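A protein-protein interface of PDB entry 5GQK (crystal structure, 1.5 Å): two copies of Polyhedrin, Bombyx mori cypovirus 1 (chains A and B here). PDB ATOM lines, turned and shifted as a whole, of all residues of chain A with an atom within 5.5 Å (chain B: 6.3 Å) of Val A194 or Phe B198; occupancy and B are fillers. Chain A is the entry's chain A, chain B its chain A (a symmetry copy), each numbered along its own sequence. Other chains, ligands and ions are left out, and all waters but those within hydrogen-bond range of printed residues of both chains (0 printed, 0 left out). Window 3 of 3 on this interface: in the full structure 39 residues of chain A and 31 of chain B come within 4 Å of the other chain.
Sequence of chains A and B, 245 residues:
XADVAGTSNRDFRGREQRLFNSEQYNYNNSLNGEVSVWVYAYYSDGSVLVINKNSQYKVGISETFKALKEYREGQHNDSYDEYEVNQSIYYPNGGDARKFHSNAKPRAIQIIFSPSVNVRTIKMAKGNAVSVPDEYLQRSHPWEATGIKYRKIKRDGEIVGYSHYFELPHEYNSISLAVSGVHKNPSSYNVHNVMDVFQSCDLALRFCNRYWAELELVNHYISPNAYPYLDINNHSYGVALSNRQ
NZ of Lys A58 is in salt-bridge range of OD2 of Asp B202 (2.7 Å).
The side-chain sulfur of Cys A201 sits at hydrogen-bond distance from the side-chain amino group of Lys A58.
The side-chain sulfur of Cys A201 lies within hydrogen-bond range of the backbone carbonyl oxygen of Val A197, at 3.5 Å.
Among the printed residues, pairs that only touch across the chains: Lys A58 with Met B195 (3.99 Å), Lys A58 with Phe B198 (3.6 Å), Val A194 with Phe B198 (3.9 Å), Val A197 with Phe B198 (3.7 Å), Phe A198 with Phe B198 (3.5 Å) and Cys A201 with Phe B198 (3.8 Å).
Val A194 touches one residue of chain B.
Phe B198 touches just these residues of chain A: Lys A58 (3.6 Å), Val A194 (3.9 Å), Val A197 (3.7 Å), Phe A198 (3.5 Å) and Cys A201 (3.8 Å).
Of the printed residues of chain A, Asp B202 touches Lys A58.
Of the printed residues of chain B, Cys A201 touches Phe B198.
Printed residues of chain B within 4 Å of Val A197: Phe B198 (3.7 Å).
Printed residues of chain B within 4 Å of Lys A58: Met B195, Phe B198 and Asp B202.
Of the printed residues of chain B, Phe A198 touches Phe B198.
Asn B193 touches none of the printed residues of chain A.
The nearest residue of chain B that does not touch Val A194 is Val B194 (4.3 Å).
The nearest printed residue of chain A that does not touch Phe B198 is Met A195 (6.1 Å).
The nearest printed residue of chain B that does not touch Cys A201 is Cys B201 (5.4 Å).
Of the 11 printed residues of chain A, 5 touch a printed residue of chain B.
Hydrophobic or aromatic side chains of chain A within 4 Å of the printed part of chain B: Val A197 and Phe A198.
Of the 11 printed residues of chain B, 3 touch a printed residue of chain A.
Among the printed residues, Asp or Glu carboxylates within 4 Å of a Lys or Arg side-chain nitrogen of the other chain: Lys A58 with Asp B202 (2.7 Å).
Val A194 touches Phe B198, but with the chains exchanged Phe A198 does not touch Val B194 (5.9 Å).
Val A197 touches Phe B198, but with the chains exchanged Phe A198 does not touch Val B197 (7.0 Å).
Phe B198 touches its own counterpart, Phe A198.
Cys A201 touches Phe B198, but with the chains exchanged Phe A198 does not touch Cys B201 (6.1 Å).
Of the 7 pairs that touch across the chains among the printed residues, 1 has its exchanged pair printed and touching as well.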
ATOM      1  N   LYS A  58      33.627 -23.211  -6.210  1.00  0.00           N
ATOM      2  CA  LYS A  58      33.100 -23.882  -5.001  1.00  0.00           C
ATOM      3  C   LYS A  58      32.553 -25.226  -5.401  1.00  0.00           C
ATOM      4  O   LYS A  58      32.191 -25.436  -6.579  1.00  0.00           O
ATOM      5  CB  LYS A  58      32.025 -22.981  -4.306  1.00  0.00           C
ATOM      6  CG  LYS A  58      30.794 -22.737  -5.173  1.00  0.00           C
ATOM      7  CD  LYS A  58      29.645 -23.646  -4.811  1.00  0.00           C
ATOM      8  CE  LYS A  58      28.546 -23.454  -5.891  1.00  0.00           C
ATOM      9  NZ  LYS A  58      27.507 -24.506  -5.672  1.00  0.00           N
ATOM     10  N   ASN A 190      36.418 -10.619  -6.854  1.00  0.00           N
ATOM     11  CA  ASN A 190      35.219 -11.491  -6.949  1.00  0.00           C
ATOM     12  C   ASN A 190      34.034 -10.778  -7.619  1.00  0.00           C
ATOM     13  O   ASN A 190      33.268 -11.389  -8.404  1.00  0.00           O
ATOM     14  CB  ASN A 190      34.827 -12.071  -5.584  1.00  0.00           C
ATOM     15  CG  ASN A 190      34.413 -11.010  -4.595  1.00  0.00           C
ATOM     16  OD1 ASN A 190      34.947  -9.903  -4.585  1.00  0.00           O
ATOM     17  ND2 ASN A 190      33.424 -11.330  -3.758  1.00  0.00           N
ATOM     18  N   HIS A 192      32.144  -8.964 -10.417  1.00  0.00           N
ATOM     19  CA  HIS A 192      32.132  -9.142 -11.835  1.00  0.00           C
ATOM     20  C   HIS A 192      31.925 -10.606 -12.176  1.00  0.00           C
ATOM     21  O   HIS A 192      31.456 -10.872 -13.288  1.00  0.00           O
ATOM     22  CB  HIS A 192      33.397  -8.638 -12.536  1.00  0.00           C
ATOM     23  CG  HIS A 192      33.483  -7.154 -12.677  1.00  0.00           C
ATOM     24  ND1 HIS A 192      34.620  -6.525 -13.177  1.00  0.00           N
ATOM     25  CD2 HIS A 192      32.599  -6.168 -12.373  1.00  0.00           C
ATOM     26  CE1 HIS A 192      34.408  -5.211 -13.191  1.00  0.00           C
ATOM     27  NE2 HIS A 192      33.225  -4.978 -12.645  1.00  0.00           N
ATOM     28  N   ASN A 193      32.249 -11.520 -11.254  1.00  0.00           N
ATOM     29  CA  ASN A 193      32.311 -12.950 -11.630  1.00  0.00           C
ATOM     30  C   ASN A 193      31.079 -13.754 -11.177  1.00  0.00           C
ATOM     31  O   ASN A 193      31.059 -14.971 -11.309  1.00  0.00           O
ATOM     32  CB  ASN A 193      33.594 -13.620 -11.079  1.00  0.00           C
ATOM     33  CG  ASN A 193      34.067 -14.782 -12.009  1.00  0.00           C
ATOM     34  OD1 ASN A 193      33.986 -14.699 -13.266  1.00  0.00           O
ATOM     35  ND2 ASN A 193      34.466 -15.881 -11.392  1.00  0.00           N
ATOM     36  N   VAL A 194      30.076 -13.099 -10.602  1.00  0.00           N
ATOM     37  CA  VAL A 194      28.943 -13.865 -10.044  1.00  0.00           C
ATOM     38  C   VAL A 194      28.199 -14.752 -11.043  1.00  0.00           C
ATOM     39  O   VAL A 194      27.904 -15.890 -10.708  1.00  0.00           O
ATOM     40  CB  VAL A 194      27.975 -12.937  -9.292  1.00  0.00           C
ATOM     41  CG1 VAL A 194      26.745 -13.704  -8.815  1.00  0.00           C
ATOM     42  CG2 VAL A 194      28.679 -12.404  -8.038  1.00  0.00           C
ATOM     43  N   MET A 195      27.960 -14.268 -12.279  1.00  0.00           N
ATOM     44  CA  MET A 195      27.283 -15.174 -13.244  1.00  0.00           C
ATOM     45  C   MET A 195      28.177 -16.371 -13.606  1.00  0.00           C
ATOM     46  O   MET A 195      27.658 -17.496 -13.890  1.00  0.00           O
ATOM     47  CB  MET A 195      26.817 -14.440 -14.463  1.00  0.00           C
ATOM     48  CG  MET A 195      25.877 -15.267 -15.355  1.00  0.00           C
ATOM     49  SD  MET A 195      24.414 -16.029 -14.538  1.00  0.00           S
ATOM     50  CE  MET A 195      23.351 -14.578 -14.557  1.00  0.00           C
ATOM     51  N   ASP A 196      29.501 -16.149 -13.563  1.00  0.00           N
ATOM     52  CA  ASP A 196      30.366 -17.303 -13.815  1.00  0.00           C
ATOM     53  C   ASP A 196      30.256 -18.362 -12.733  1.00  0.00           C
ATOM     54  O   ASP A 196      30.340 -19.566 -13.010  1.00  0.00           O
ATOM     55  CB  ASP A 196      31.830 -16.885 -13.974  1.00  0.00           C
ATOM     56  CG  ASP A 196      32.090 -16.245 -15.310  1.00  0.00           C
ATOM     57  OD1 ASP A 196      31.326 -15.309 -15.627  1.00  0.00           O
ATOM     58  OD2 ASP A 196      33.003 -16.674 -16.039  1.00  0.00           O
ATOM     59  N   VAL A 197      30.069 -17.908 -11.501  1.00  0.00           N
ATOM     60  CA  VAL A 197      29.854 -18.881 -10.437  1.00  0.00           C
ATOM     61  C   VAL A 197      28.497 -19.576 -10.592  1.00  0.00           C
ATOM     62  O   VAL A 197      28.399 -20.822 -10.356  1.00  0.00           O
ATOM     63  CB  VAL A 197      30.065 -18.270  -9.007  1.00  0.00           C
ATOM     64  CG1 VAL A 197      29.971 -19.391  -7.920  1.00  0.00           C
ATOM     65  CG2 VAL A 197      31.444 -17.548  -8.936  1.00  0.00           C
ATOM     66  N   PHE A 198      27.480 -18.830 -11.066  1.00  0.00           N
ATOM     67  CA  PHE A 198      26.230 -19.531 -11.348  1.00  0.00           C
ATOM     68  C   PHE A 198      26.422 -20.577 -12.417  1.00  0.00           C
ATOM     69  O   PHE A 198      25.892 -21.699 -12.314  1.00  0.00           O
ATOM     70  CB  PHE A 198      25.086 -18.560 -11.785  1.00  0.00           C
ATOM     71  CG  PHE A 198      24.385 -17.882 -10.617  1.00  0.00           C
ATOM     72  CD1 PHE A 198      23.606 -18.645  -9.740  1.00  0.00           C
ATOM     73  CD2 PHE A 198      24.574 -16.494 -10.391  1.00  0.00           C
ATOM     74  CE1 PHE A 198      22.968 -18.050  -8.644  1.00  0.00           C
ATOM     75  CE2 PHE A 198      23.926 -15.892  -9.335  1.00  0.00           C
ATOM     76  CZ  PHE A 198      23.184 -16.695  -8.452  1.00  0.00           C
ATOM     77  N   GLN A 199      27.157 -20.244 -13.480  1.00  0.00           N
ATOM     78  CA  GLN A 199      27.432 -21.273 -14.477  1.00  0.00           C
ATOM     79  C   GLN A 199      28.231 -22.448 -13.914  1.00  0.00           C
ATOM     80  O   GLN A 199      27.977 -23.585 -14.313  1.00  0.00           O
ATOM     81  CB  GLN A 199      28.154 -20.689 -15.665  1.00  0.00           C
ATOM     82  CG  GLN A 199      27.308 -19.737 -16.496  1.00  0.00           C
ATOM     83  CD  GLN A 199      27.971 -19.495 -17.863  1.00  0.00           C
ATOM     84  OE1 GLN A 199      28.772 -18.539 -18.002  1.00  0.00           O
ATOM     85  NE2 GLN A 199      27.591 -20.314 -18.881  1.00  0.00           N
ATOM     86  N   CYS A 201      27.788 -23.819 -11.140  1.00  0.00           N
ATOM     87  CA  CYS A 201      26.790 -24.720 -10.508  1.00  0.00           C
ATOM     88  C   CYS A 201      26.271 -25.702 -11.573  1.00  0.00           C
ATOM     89  O   CYS A 201      26.009 -26.822 -11.216  1.00  0.00           O
ATOM     90  CB  CYS A 201      25.625 -23.904  -9.972  1.00  0.00           C
ATOM     91  SG  CYS A 201      26.099 -22.856  -8.579  1.00  0.00           S
ATOM     92  N   ASN B 193      27.774 -11.554   1.274  1.00  0.00           N
ATOM     93  CA  ASN B 193      27.361 -12.927   1.643  1.00  0.00           C
ATOM     94  C   ASN B 193      27.098 -13.832   0.426  1.00  0.00           C
ATOM     95  O   ASN B 193      26.627 -14.951   0.586  1.00  0.00           O
ATOM     96  CB  ASN B 193      26.109 -12.911   2.553  1.00  0.00           C
ATOM     97  CG  ASN B 193      26.102 -14.135   3.524  1.00  0.00           C
ATOM     98  OD1 ASN B 193      27.163 -14.565   4.055  1.00  0.00           O
ATOM     99  ND2 ASN B 193      24.935 -14.738   3.672  1.00  0.00           N
ATOM    100  N   VAL B 194      27.348 -13.348  -0.786  1.00  0.00           N
ATOM    101  CA  VAL B 194      26.982 -14.150  -1.971  1.00  0.00           C
ATOM    102  C   VAL B 194      27.633 -15.532  -2.051  1.00  0.00           C
ATOM    103  O   VAL B 194      26.939 -16.488  -2.364  1.00  0.00           O
ATOM    104  CB  VAL B 194      27.210 -13.350  -3.263  1.00  0.00           C
ATOM    105  CG1 VAL B 194      26.945 -14.213  -4.493  1.00  0.00           C
ATOM    106  CG2 VAL B 194      26.203 -12.193  -3.308  1.00  0.00           C
ATOM    107  N   MET B 195      28.931 -15.652  -1.704  1.00  0.00           N
ATOM    108  CA  MET B 195      29.520 -17.016  -1.741  1.00  0.00           C
ATOM    109  C   MET B 195      28.886 -17.926  -0.677  1.00  0.00           C
ATOM    110  O   MET B 195      28.773 -19.175  -0.886  1.00  0.00           O
ATOM    111  CB  MET B 195      31.013 -16.981  -1.623  1.00  0.00           C
ATOM    112  CG  MET B 195      31.684 -18.329  -1.931  1.00  0.00           C
ATOM    113  SD  MET B 195      31.244 -19.130  -3.529  1.00  0.00           S
ATOM    114  CE  MET B 195      32.366 -18.195  -4.579  1.00  0.00           C
ATOM    115  N   ASP B 196      28.444 -17.312   0.433  1.00  0.00           N
ATOM    116  CA  ASP B 196      27.755 -18.152   1.414  1.00  0.00           C
ATOM    117  C   ASP B 196      26.439 -18.699   0.892  1.00  0.00           C
ATOM    118  O   ASP B 196      26.048 -19.830   1.212  1.00  0.00           O
ATOM    119  CB  ASP B 196      27.512 -17.400   2.727  1.00  0.00           C
ATOM    120  CG  ASP B 196      28.769 -17.270   3.540  1.00  0.00           C
ATOM    121  OD1 ASP B 196      29.763 -16.807   2.943  1.00  0.00           O
ATOM    122  OD2 ASP B 196      28.784 -17.644   4.728  1.00  0.00           O
ATOM    123  N   VAL B 197      25.758 -17.891   0.090  1.00  0.00           N
ATOM    124  CA  VAL B 197      24.538 -18.402  -0.523  1.00  0.00           C
ATOM    125  C   VAL B 197      24.854 -19.481  -1.563  1.00  0.00           C
ATOM    126  O   VAL B 197      24.110 -20.509  -1.647  1.00  0.00           O
ATOM    127  CB  VAL B 197      23.622 -17.260  -1.089  1.00  0.00           C
ATOM    128  CG1 VAL B 197      22.266 -17.854  -1.594  1.00  0.00           C
ATOM    129  CG2 VAL B 197      23.376 -16.182   0.009  1.00  0.00           C
ATOM    130  N   PHE B 198      25.979 -19.321  -2.287  1.00  0.00           N
ATOM    131  CA  PHE B 198      26.351 -20.421  -3.172  1.00  0.00           C
ATOM    132  C   PHE B 198      26.618 -21.682  -2.390  1.00  0.00           C
ATOM    133  O   PHE B 198      26.206 -22.785  -2.796  1.00  0.00           O
ATOM    134  CB  PHE B 198      27.604 -20.089  -4.045  1.00  0.00           C
ATOM    135  CG  PHE B 198      27.281 -19.266  -5.284  1.00  0.00           C
ATOM    136  CD1 PHE B 198      26.528 -19.837  -6.316  1.00  0.00           C
ATOM    137  CD2 PHE B 198      27.694 -17.911  -5.358  1.00  0.00           C
ATOM    138  CE1 PHE B 198      26.197 -19.095  -7.457  1.00  0.00           C
ATOM    139  CE2 PHE B 198      27.402 -17.181  -6.489  1.00  0.00           C
ATOM    140  CZ  PHE B 198      26.610 -17.773  -7.488  1.00  0.00           C
ATOM    141  N   GLN B 199      27.330 -21.571  -1.266  1.00  0.00           N
ATOM    142  CA  GLN B 199      27.516 -22.765  -0.448  1.00  0.00           C
ATOM    143  C   GLN B 199      26.200 -23.333   0.082  1.00  0.00           C
ATOM    144  O   GLN B 199      26.069 -24.555   0.161  1.00  0.00           O
ATOM    145  CB  GLN B 199      28.451 -22.486   0.702  1.00  0.00           C
ATOM    146  CG  GLN B 199      29.889 -22.229   0.281  1.00  0.00           C
ATOM    147  CD  GLN B 199      30.823 -22.335   1.498  1.00  0.00           C
ATOM    148  OE1 GLN B 199      31.080 -21.309   2.173  1.00  0.00           O
ATOM    149  NE2 GLN B 199      31.381 -23.553   1.737  1.00  0.00           N
ATOM    150  N   SER B 200      25.217 -22.478   0.393  1.00  0.00           N
ATOM    151  CA  SER B 200      23.922 -22.991   0.833  1.00  0.00           C
ATOM    152  C   SER B 200      23.245 -23.867  -0.232  1.00  0.00           C
ATOM    153  O   SER B 200      22.549 -24.786   0.136  1.00  0.00           O
ATOM    154  CB  SER B 200      23.017 -21.819   1.280  1.00  0.00           C
ATOM    155  OG  SER B 200      22.315 -21.237   0.161  1.00  0.00           O
ATOM    156  N   CYS B 201      23.531 -23.612  -1.520  1.00  0.00           N
ATOM    157  CA  CYS B 201      22.989 -24.462  -2.611  1.00  0.00           C
ATOM    158  C   CYS B 201      23.560 -25.883  -2.455  1.00  0.00           C
ATOM    159  O   CYS B 201      22.845 -26.805  -2.752  1.00  0.00           O
ATOM    160  CB  CYS B 201      23.410 -23.902  -3.961  1.00  0.00           C
ATOM    161  SG  CYS B 201      22.630 -22.312  -4.320  1.00  0.00           S
ATOM    162  N   ASP B 202      24.803 -26.064  -1.992  1.00  0.00           N
ATOM    163  CA  ASP B 202      25.336 -27.383  -1.826  1.00  0.00           C
ATOM    164  C   ASP B 202      24.923 -27.990  -0.492  1.00  0.00           C
ATOM    165  O   ASP B 202      24.860 -29.220  -0.384  1.00  0.00           O
ATOM    166  CB  ASP B 202      26.839 -27.344  -1.926  1.00  0.00           C
ATOM    167  CG  ASP B 202      27.292 -27.235  -3.362  1.00  0.00           C
ATOM    168  OD1 ASP B 202      26.903 -28.095  -4.183  1.00  0.00           O
ATOM    169  OD2 ASP B 202      28.008 -26.293  -3.669  1.00  0.00           O
ATOM    170  N   LEU B 203      24.706 -27.136   0.502  1.00  0.00           N
ATOM    171  CA  LEU B 203      24.443 -27.569   1.867  1.00  0.00           C
ATOM    172  C   LEU B 203      22.978 -27.956   2.160  1.00  0.00           C
ATOM    173  O   LEU B 203      22.676 -28.620   3.201  1.00  0.00           O
ATOM    174  CB  LEU B 203      24.924 -26.516   2.881  1.00  0.00           C
ATOM    175  CG  LEU B 203      26.462 -26.407   2.928  1.00  0.00           C
ATOM    176  CD1 LEU B 203      26.911 -25.060   3.528  1.00  0.00           C
ATOM    177  CD2 LEU B 203      27.070 -27.623   3.670  1.00  0.00           C
